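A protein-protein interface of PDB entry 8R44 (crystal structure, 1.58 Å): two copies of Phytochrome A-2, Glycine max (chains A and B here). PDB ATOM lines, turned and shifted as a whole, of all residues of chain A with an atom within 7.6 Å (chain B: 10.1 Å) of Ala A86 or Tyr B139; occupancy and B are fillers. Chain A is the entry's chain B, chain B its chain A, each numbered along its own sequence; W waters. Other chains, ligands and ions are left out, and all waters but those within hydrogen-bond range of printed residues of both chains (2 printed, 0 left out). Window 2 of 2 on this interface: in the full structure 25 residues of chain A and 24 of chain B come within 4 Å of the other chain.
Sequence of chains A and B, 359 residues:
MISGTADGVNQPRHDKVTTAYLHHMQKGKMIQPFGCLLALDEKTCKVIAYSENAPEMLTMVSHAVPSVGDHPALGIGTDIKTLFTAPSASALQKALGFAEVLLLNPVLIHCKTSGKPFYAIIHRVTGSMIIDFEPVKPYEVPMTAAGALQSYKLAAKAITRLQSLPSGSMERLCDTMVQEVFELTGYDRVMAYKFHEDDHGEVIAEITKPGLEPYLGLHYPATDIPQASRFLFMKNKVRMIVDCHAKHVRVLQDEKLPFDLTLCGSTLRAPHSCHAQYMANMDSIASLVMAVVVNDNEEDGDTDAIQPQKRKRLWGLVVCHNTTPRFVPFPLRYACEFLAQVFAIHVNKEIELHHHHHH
Printed residues of chain B that touch a printed residue of chain A: Tyr B139 and Pro B142.
Hydrophobic or aromatic side chains of chain B that line the printed part of chain A: Tyr B139 and Pro B142.
Of the 15 printed residues of chain A, 4 touch a printed residue of chain B.
Hydrophobic or aromatic side chains of chain A that line the printed part of chain B: Ala A86 and Ala A91.
Position printed for both chains: 110.
Of the 5 pairs that touch across the chains among the printed residues, none has its exchanged pair printed and touching as well.
CB of Ala A86 touches OH of Tyr B139 (3.8 Å).
Tyr B139 touches Pro A87.
Pro A87 touches Pro B142.
Ser A90 touches Tyr B139 (CB to CE2, 3.5 Å).
CB of Pro B142 touches CB of Ala A91, 3.9 Å away.
Printed residues of chain B within 4 Å of Ala A86: Tyr B139 (3.8 Å).
Of the printed residues of chain A, Tyr B139 touches Ala A86, Pro A87 and Ser A90.
No residue of chain B comes within 4 Å of Thr A85.
Pro A87 touches just these residues of chain B: Tyr B139 and Pro B142.
No residue of chain B comes within 4 Å of Ser A88.
Printed residues of chain B within 4 Å of Ala A91: Pro B142.
Of the printed residues of chain B, Ser A90 touches Tyr B139.
Of the printed residues of chain A, Pro B142 touches Pro A87 and Ala A91.
Lys B137 touches none of the printed residues of chain A.
The nearest residue of chain B that does not touch Ala A86 is Pro B142 (6.9 Å).
The nearest printed residue of chain B that does not touch Ala A91 is Met B143 (4.5 Å).
Water W1 lies within hydrogen-bond range of O of Tyr B139 (2.7 Å), O of Pro A87 (2.9 Å) and N of Ala A91 (3.4 Å).
Water W2 lies within hydrogen-bond range of the backbone carbonyl oxygen of Ala A91 (2.8 Å) and the side-chain sulfur of Met B143 (3.4 Å).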
ATOM      1  N   ILE A  80      12.300  43.009  -3.102  1.00  0.00           N
ATOM      2  CA  ILE A  80      12.885  41.905  -2.338  1.00  0.00           C
ATOM      3  C   ILE A  80      13.874  41.097  -3.170  1.00  0.00           C
ATOM      4  O   ILE A  80      14.664  40.361  -2.591  1.00  0.00           O
ATOM      5  CB  ILE A  80      11.841  40.994  -1.703  1.00  0.00           C
ATOM      6  CG1 ILE A  80      10.990  40.235  -2.722  1.00  0.00           C
ATOM      7  CG2 ILE A  80      10.958  41.829  -0.765  1.00  0.00           C
ATOM      8  CD1 ILE A  80      10.102  39.173  -2.133  1.00  0.00           C
ATOM      9  N   LYS A  81      13.880  41.242  -4.501  1.00  0.00           N
ATOM     10  CA  LYS A  81      14.895  40.556  -5.296  1.00  0.00           C
ATOM     11  C   LYS A  81      16.280  41.103  -5.055  1.00  0.00           C
ATOM     12  O   LYS A  81      17.259  40.442  -5.404  1.00  0.00           O
ATOM     13  CB  LYS A  81      14.544  40.669  -6.782  1.00  0.00           C
ATOM     14  CG  LYS A  81      13.268  39.937  -7.150  1.00  0.00           C
ATOM     15  CD  LYS A  81      12.956  39.926  -8.623  1.00  0.00           C
ATOM     16  CE  LYS A  81      12.755  41.316  -9.162  1.00  0.00           C
ATOM     17  NZ  LYS A  81      11.583  41.942  -8.493  1.00  0.00           N
ATOM     18  N   LEU A  83      17.220  41.678  -1.908  1.00  0.00           N
ATOM     19  CA  LEU A  83      17.497  41.323  -0.517  1.00  0.00           C
ATOM     20  C   LEU A  83      17.827  39.844  -0.361  1.00  0.00           C
ATOM     21  O   LEU A  83      18.640  39.533   0.494  1.00  0.00           O
ATOM     22  CB  LEU A  83      16.263  41.600   0.333  1.00  0.00           C
ATOM     23  CG  LEU A  83      15.829  43.063   0.455  1.00  0.00           C
ATOM     24  CD1 LEU A  83      14.558  43.155   1.310  1.00  0.00           C
ATOM     25  CD2 LEU A  83      16.931  43.948   1.015  1.00  0.00           C
ATOM     26  N   PHE A  84      17.215  38.981  -1.183  1.00  0.00           N
ATOM     27  CA  PHE A  84      17.272  37.548  -0.999  1.00  0.00           C
ATOM     28  C   PHE A  84      17.786  36.891  -2.269  1.00  0.00           C
ATOM     29  O   PHE A  84      17.687  37.451  -3.354  1.00  0.00           O
ATOM     30  CB  PHE A  84      15.894  36.995  -0.643  1.00  0.00           C
ATOM     31  CG  PHE A  84      15.246  37.743   0.499  1.00  0.00           C
ATOM     32  CD1 PHE A  84      15.876  37.835   1.719  1.00  0.00           C
ATOM     33  CD2 PHE A  84      14.086  38.462   0.344  1.00  0.00           C
ATOM     34  CE1 PHE A  84      15.318  38.511   2.770  1.00  0.00           C
ATOM     35  CE2 PHE A  84      13.513  39.125   1.412  1.00  0.00           C
ATOM     36  CZ  PHE A  84      14.143  39.186   2.626  1.00  0.00           C
ATOM     37  N   THR A  85      18.309  35.680  -2.146  1.00  0.00           N
ATOM     38  CA  THR A  85      18.641  34.890  -3.326  1.00  0.00           C
ATOM     39  C   THR A  85      17.408  34.621  -4.194  1.00  0.00           C
ATOM     40  O   THR A  85      16.255  34.700  -3.762  1.00  0.00           O
ATOM     41  CB  THR A  85      19.259  33.535  -2.993  1.00  0.00           C
ATOM     42  OG1 THR A  85      18.287  32.723  -2.339  1.00  0.00           O
ATOM     43  CG2 THR A  85      20.523  33.676  -2.159  1.00  0.00           C
ATOM     44  N   ALA A  86      17.640  34.287  -5.465  1.00  0.00           N
ATOM     45  CA  ALA A  86      16.511  34.225  -6.379  1.00  0.00           C
ATOM     46  C   ALA A  86      15.421  33.237  -5.935  1.00  0.00           C
ATOM     47  O   ALA A  86      14.226  33.580  -5.927  1.00  0.00           O
ATOM     48  CB  ALA A  86      16.977  33.966  -7.805  1.00  0.00           C
ATOM     49  N   PRO A  87      15.747  31.989  -5.524  1.00  0.00           N
ATOM     50  CA  PRO A  87      14.710  31.062  -5.093  1.00  0.00           C
ATOM     51  C   PRO A  87      13.995  31.546  -3.835  1.00  0.00           C
ATOM     52  O   PRO A  87      12.819  31.260  -3.670  1.00  0.00           O
ATOM     53  CB  PRO A  87      15.470  29.752  -4.834  1.00  0.00           C
ATOM     54  CG  PRO A  87      16.696  29.920  -5.671  1.00  0.00           C
ATOM     55  CD  PRO A  87      17.079  31.375  -5.535  1.00  0.00           C
ATOM     56  N   SER A  88      14.714  32.268  -2.974  1.00  0.00           N
ATOM     57  CA  SER A  88      14.120  32.804  -1.749  1.00  0.00           C
ATOM     58  C   SER A  88      13.102  33.897  -2.101  1.00  0.00           C
ATOM     59  O   SER A  88      11.984  33.911  -1.584  1.00  0.00           O
ATOM     60  CB  SER A  88      15.208  33.328  -0.843  1.00  0.00           C
ATOM     61  OG  SER A  88      15.897  32.260  -0.211  1.00  0.00           O
ATOM     62  N   ALA A  89      13.543  34.864  -2.907  1.00  0.00           N
ATOM     63  CA  ALA A  89      12.677  35.967  -3.315  1.00  0.00           C
ATOM     64  C   ALA A  89      11.432  35.444  -4.000  1.00  0.00           C
ATOM     65  O   ALA A  89      10.305  35.900  -3.753  1.00  0.00           O
ATOM     66  CB  ALA A  89      13.436  36.933  -4.170  1.00  0.00           C
ATOM     67  N   SER A  90      11.602  34.407  -4.820  1.00  0.00           N
ATOM     68  CA  SER A  90      10.485  33.844  -5.571  1.00  0.00           C
ATOM     69  C   SER A  90       9.497  33.161  -4.640  1.00  0.00           C
ATOM     70  O   SER A  90       8.268  33.296  -4.786  1.00  0.00           O
ATOM     71  CB  SER A  90      10.983  32.918  -6.645  1.00  0.00           C
ATOM     72  OG  SER A  90       9.886  32.288  -7.325  1.00  0.00           O
ATOM     73  N   ALA A  91      10.025  32.422  -3.641  1.00  0.00           N
ATOM     74  CA  ALA A  91       9.141  31.768  -2.691  1.00  0.00           C
ATOM     75  C   ALA A  91       8.275  32.800  -1.964  1.00  0.00           C
ATOM     76  O   ALA A  91       7.108  32.535  -1.712  1.00  0.00           O
ATOM     77  CB  ALA A  91       9.923  30.910  -1.721  1.00  0.00           C
ATOM     78  N   LEU A  92       8.851  33.951  -1.592  1.00  0.00           N
ATOM     79  CA  LEU A  92       8.065  34.967  -0.911  1.00  0.00           C
ATOM     80  C   LEU A  92       7.036  35.571  -1.874  1.00  0.00           C
ATOM     81  O   LEU A  92       5.886  35.738  -1.483  1.00  0.00           O
ATOM     82  CB  LEU A  92       8.988  36.026  -0.316  1.00  0.00           C
ATOM     83  CG  LEU A  92       9.959  35.498   0.734  1.00  0.00           C
ATOM     84  CD1 LEU A  92      10.817  36.645   1.225  1.00  0.00           C
ATOM     85  CD2 LEU A  92       9.235  34.826   1.900  1.00  0.00           C
ATOM     86  N   LYS A  94       5.638  34.174  -4.474  1.00  0.00           N
ATOM     87  CA  LYS A  94       4.591  33.187  -4.723  1.00  0.00           C
ATOM     88  C   LYS A  94       3.607  33.081  -3.563  1.00  0.00           C
ATOM     89  O   LYS A  94       2.450  32.673  -3.755  1.00  0.00           O
ATOM     90  CB  LYS A  94       5.158  31.801  -5.039  1.00  0.00           C
ATOM     91  CG  LYS A  94       5.851  31.709  -6.403  1.00  0.00           C
ATOM     92  CD  LYS A  94       5.026  32.200  -7.605  1.00  0.00           C
ATOM     93  CE  LYS A  94       5.837  32.521  -8.851  1.00  0.00           C
ATOM     94  NZ  LYS A  94       5.946  31.385  -9.801  1.00  0.00           N
ATOM     95  N   HIS A 110      17.533  32.688   2.196  1.00  0.00           N
ATOM     96  CA  HIS A 110      18.913  33.150   2.256  1.00  0.00           C
ATOM     97  C   HIS A 110      19.014  34.594   1.770  1.00  0.00           C
ATOM     98  O   HIS A 110      18.488  34.965   0.712  1.00  0.00           O
ATOM     99  CB  HIS A 110      19.856  32.218   1.463  1.00  0.00           C
ATOM    100  CG  HIS A 110      19.949  30.859   2.039  1.00  0.00           C
ATOM    101  ND1 HIS A 110      21.005  30.445   2.817  1.00  0.00           N
ATOM    102  CD2 HIS A 110      19.092  29.846   2.013  1.00  0.00           C
ATOM    103  CE1 HIS A 110      20.791  29.169   3.211  1.00  0.00           C
ATOM    104  NE2 HIS A 110      19.603  28.804   2.726  1.00  0.00           N
ATOM    105  N   LYS A 112      20.822  37.708   0.055  1.00  0.00           N
ATOM    106  CA  LYS A 112      21.514  37.736  -1.206  1.00  0.00           C
ATOM    107  C   LYS A 112      23.007  37.984  -1.001  1.00  0.00           C
ATOM    108  O   LYS A 112      23.804  37.329  -1.655  1.00  0.00           O
ATOM    109  CB  LYS A 112      20.932  38.861  -2.049  1.00  0.00           C
ATOM    110  CG  LYS A 112      21.506  38.967  -3.455  1.00  0.00           C
ATOM    111  CD  LYS A 112      20.726  39.967  -4.260  1.00  0.00           C
ATOM    112  CE  LYS A 112      20.790  39.799  -5.760  1.00  0.00           C
ATOM    113  NZ  LYS A 112      22.189  39.834  -6.219  1.00  0.00           N
ATOM    114  N   LEU B 108      18.937  17.769   3.743  1.00  0.00           N
ATOM    115  CA  LEU B 108      18.860  18.444   2.462  1.00  0.00           C
ATOM    116  C   LEU B 108      20.263  18.783   2.007  1.00  0.00           C
ATOM    117  O   LEU B 108      20.943  19.579   2.666  1.00  0.00           O
ATOM    118  CB  LEU B 108      17.967  19.705   2.544  1.00  0.00           C
ATOM    119  CG  LEU B 108      17.511  20.359   1.208  1.00  0.00           C
ATOM    120  CD1 LEU B 108      18.620  20.914   0.348  1.00  0.00           C
ATOM    121  CD2 LEU B 108      16.714  19.393   0.365  1.00  0.00           C
ATOM    122  N   HIS B 110      23.051  19.795  -1.248  1.00  0.00           N
ATOM    123  CA  HIS B 110      23.286  20.458  -2.517  1.00  0.00           C
ATOM    124  C   HIS B 110      24.605  19.986  -3.125  1.00  0.00           C
ATOM    125  O   HIS B 110      25.638  19.892  -2.442  1.00  0.00           O
ATOM    126  CB  HIS B 110      23.355  21.989  -2.389  1.00  0.00           C
ATOM    127  CG  HIS B 110      22.100  22.599  -1.935  1.00  0.00           C
ATOM    128  ND1 HIS B 110      21.185  23.109  -2.834  1.00  0.00           N
ATOM    129  CD2 HIS B 110      21.583  22.746  -0.733  1.00  0.00           C
ATOM    130  CE1 HIS B 110      20.145  23.563  -2.159  1.00  0.00           C
ATOM    131  NE2 HIS B 110      20.338  23.351  -0.862  1.00  0.00           N
ATOM    132  N   SER B 114      26.706  23.507  -8.872  1.00  0.00           N
ATOM    133  CA  SER B 114      25.346  23.557  -9.417  1.00  0.00           C
ATOM    134  C   SER B 114      24.302  23.920  -8.367  1.00  0.00           C
ATOM    135  O   SER B 114      23.252  24.490  -8.683  1.00  0.00           O
ATOM    136  CB  SER B 114      24.960  22.221 -10.022  1.00  0.00           C
ATOM    137  OG  SER B 114      24.925  21.210  -9.009  1.00  0.00           O
ATOM    138  N   GLY B 115      24.567  23.530  -7.114  1.00  0.00           N
ATOM    139  CA  GLY B 115      23.583  23.593  -6.063  1.00  0.00           C
ATOM    140  C   GLY B 115      22.467  22.567  -6.273  1.00  0.00           C
ATOM    141  O   GLY B 115      21.422  22.689  -5.643  1.00  0.00           O
ATOM    142  N   LYS B 116      22.656  21.600  -7.177  1.00  0.00           N
ATOM    143  CA  LYS B 116      21.549  20.678  -7.451  1.00  0.00           C
ATOM    144  C   LYS B 116      21.105  19.971  -6.154  1.00  0.00           C
ATOM    145  O   LYS B 116      21.922  19.371  -5.455  1.00  0.00           O
ATOM    146  CB  LYS B 116      21.971  19.648  -8.485  1.00  0.00           C
ATOM    147  CG  LYS B 116      20.880  18.756  -9.016  1.00  0.00           C
ATOM    148  CD  LYS B 116      21.400  17.700  -9.971  1.00  0.00           C
ATOM    149  CE  LYS B 116      20.272  16.862 -10.526  1.00  0.00           C
ATOM    150  NZ  LYS B 116      20.823  15.901 -11.496  1.00  0.00           N
ATOM    151  N   PRO B 117      19.831  20.045  -5.744  1.00  0.00           N
ATOM    152  CA  PRO B 117      19.462  19.535  -4.422  1.00  0.00           C
ATOM    153  C   PRO B 117      18.824  18.149  -4.397  1.00  0.00           C
ATOM    154  O   PRO B 117      18.139  17.757  -5.341  1.00  0.00           O
ATOM    155  CB  PRO B 117      18.422  20.570  -3.981  1.00  0.00           C
ATOM    156  CG  PRO B 117      17.701  20.931  -5.263  1.00  0.00           C
ATOM    157  CD  PRO B 117      18.770  20.890  -6.320  1.00  0.00           C
ATOM    158  N   PRO B 135      16.007  13.281  -5.712  1.00  0.00           N
ATOM    159  CA  PRO B 135      16.005  14.677  -6.165  1.00  0.00           C
ATOM    160  C   PRO B 135      14.843  15.491  -5.617  1.00  0.00           C
ATOM    161  O   PRO B 135      13.730  14.996  -5.369  1.00  0.00           O
ATOM    162  CB  PRO B 135      15.920  14.619  -7.687  1.00  0.00           C
ATOM    163  CG  PRO B 135      15.673  13.181  -8.031  1.00  0.00           C
ATOM    164  CD  PRO B 135      15.890  12.325  -6.814  1.00  0.00           C
ATOM    165  N   VAL B 136      15.116  16.794  -5.499  1.00  0.00           N
ATOM    166  CA  VAL B 136      14.163  17.820  -5.111  1.00  0.00           C
ATOM    167  C   VAL B 136      14.134  18.900  -6.193  1.00  0.00           C
ATOM    168  O   VAL B 136      15.165  19.244  -6.739  1.00  0.00           O
ATOM    169  CB  VAL B 136      14.531  18.445  -3.756  1.00  0.00           C
ATOM    170  CG1 VAL B 136      13.578  19.587  -3.386  1.00  0.00           C
ATOM    171  CG2 VAL B 136      14.499  17.359  -2.678  1.00  0.00           C
ATOM    172  N   LYS B 137      12.945  19.423  -6.489  1.00  0.00           N
ATOM    173  CA  LYS B 137      12.849  20.506  -7.462  1.00  0.00           C
ATOM    174  C   LYS B 137      13.522  21.735  -6.837  1.00  0.00           C
ATOM    175  O   LYS B 137      13.183  22.130  -5.733  1.00  0.00           O
ATOM    176  CB  LYS B 137      11.368  20.698  -7.819  1.00  0.00           C
ATOM    177  CG  LYS B 137      11.098  21.907  -8.668  1.00  0.00           C
ATOM    178  CD  LYS B 137       9.703  21.903  -9.232  1.00  0.00           C
ATOM    179  CE  LYS B 137       9.465  23.102 -10.128  1.00  0.00           C
ATOM    180  NZ  LYS B 137       8.006  23.404 -10.265  1.00  0.00           N
ATOM    181  N   PRO B 138      14.501  22.379  -7.499  1.00  0.00           N
ATOM    182  CA  PRO B 138      15.278  23.454  -6.906  1.00  0.00           C
ATOM    183  C   PRO B 138      14.486  24.599  -6.305  1.00  0.00           C
ATOM    184  O   PRO B 138      14.786  24.993  -5.179  1.00  0.00           O
ATOM    185  CB  PRO B 138      16.166  23.960  -8.065  1.00  0.00           C
ATOM    186  CG  PRO B 138      16.331  22.778  -8.937  1.00  0.00           C
ATOM    187  CD  PRO B 138      15.044  21.996  -8.813  1.00  0.00           C
ATOM    188  N   TYR B 139      13.447  25.075  -6.993  1.00  0.00           N
ATOM    189  CA  TYR B 139      12.685  26.192  -6.432  1.00  0.00           C
ATOM    190  C   TYR B 139      11.802  25.766  -5.252  1.00  0.00           C
ATOM    191  O   TYR B 139      11.215  26.642  -4.582  1.00  0.00           O
ATOM    192  CB  TYR B 139      11.890  26.990  -7.473  1.00  0.00           C
ATOM    193  CG  TYR B 139      12.667  28.159  -8.030  1.00  0.00           C
ATOM    194  CD1 TYR B 139      13.847  27.989  -8.720  1.00  0.00           C
ATOM    195  CD2 TYR B 139      12.182  29.448  -7.916  1.00  0.00           C
ATOM    196  CE1 TYR B 139      14.607  29.063  -9.180  1.00  0.00           C
ATOM    197  CE2 TYR B 139      12.922  30.515  -8.378  1.00  0.00           C
ATOM    198  CZ  TYR B 139      14.128  30.328  -9.023  1.00  0.00           C
ATOM    199  OH  TYR B 139      14.727  31.457  -9.486  1.00  0.00           O
ATOM    200  N   GLU B 140      11.712  24.459  -4.958  1.00  0.00           N
ATOM    201  CA  GLU B 140      10.980  24.007  -3.778  1.00  0.00           C
ATOM    202  C   GLU B 140      11.884  23.951  -2.540  1.00  0.00           C
ATOM    203  O   GLU B 140      11.356  23.712  -1.463  1.00  0.00           O
ATOM    204  CB  GLU B 140      10.324  22.642  -4.000  1.00  0.00           C
ATOM    205  CG  GLU B 140       9.223  22.674  -5.066  1.00  0.00           C
ATOM    206  CD  GLU B 140       8.490  21.374  -5.317  1.00  0.00           C
ATOM    207  OE1 GLU B 140       8.821  20.337  -4.654  1.00  0.00           O
ATOM    208  OE2 GLU B 140       7.509  21.427  -6.112  1.00  0.00           O
ATOM    209  N   VAL B 141      13.203  24.104  -2.688  1.00  0.00           N
ATOM    210  CA  VAL B 141      14.105  23.986  -1.555  1.00  0.00           C
ATOM    211  C   VAL B 141      13.694  24.918  -0.408  1.00  0.00           C
ATOM    212  O   VAL B 141      13.676  24.490   0.747  1.00  0.00           O
ATOM    213  CB  VAL B 141      15.578  24.138  -1.956  1.00  0.00           C
ATOM    214  CG1 VAL B 141      16.463  24.321  -0.730  1.00  0.00           C
ATOM    215  CG2 VAL B 141      16.033  22.909  -2.738  1.00  0.00           C
ATOM    216  N   PRO B 142      13.320  26.191  -0.644  1.00  0.00           N
ATOM    217  CA  PRO B 142      12.894  27.059   0.463  1.00  0.00           C
ATOM    218  C   PRO B 142      11.710  26.526   1.263  1.00  0.00           C
ATOM    219  O   PRO B 142      11.498  26.966   2.402  1.00  0.00           O
ATOM    220  CB  PRO B 142      12.563  28.403  -0.229  1.00  0.00           C
ATOM    221  CG  PRO B 142      13.406  28.331  -1.504  1.00  0.00           C
ATOM    222  CD  PRO B 142      13.305  26.895  -1.958  1.00  0.00           C
ATOM    223  N   MET B 143      10.891  25.665   0.663  1.00  0.00           N
ATOM    224  CA  MET B 143       9.687  25.167   1.284  1.00  0.00           C
ATOM    225  C   MET B 143       9.877  23.769   1.904  1.00  0.00           C
ATOM    226  O   MET B 143       8.893  23.119   2.267  1.00  0.00           O
ATOM    227  CB  MET B 143       8.578  25.097   0.230  1.00  0.00           C
ATOM    228  CG  MET B 143       8.306  26.417  -0.459  1.00  0.00           C
ATOM    229  SD  MET B 143       7.890  27.723   0.688  1.00  0.00           S
ATOM    230  CE  MET B 143       6.334  27.168   1.407  1.00  0.00           C
ATOM    231  N   THR B 144      11.114  23.284   2.107  1.00  0.00           N
ATOM    232  CA  THR B 144      11.281  21.906   2.536  1.00  0.00           C
ATOM    233  C   THR B 144      10.717  21.694   3.954  1.00  0.00           C
ATOM    234  O   THR B 144       9.995  20.727   4.186  1.00  0.00           O
ATOM    235  CB  THR B 144      12.737  21.439   2.398  1.00  0.00           C
ATOM    236  OG1 THR B 144      13.560  22.313   3.114  1.00  0.00           O
ATOM    237  CG2 THR B 144      13.259  21.490   1.002  1.00  0.00           C
HETATM  238  O   HOH W   1      10.961  29.314  -4.626  1.00  0.00           O
HETATM  239  O   HOH W   2       6.033  30.030  -1.024  1.00  0.00           O
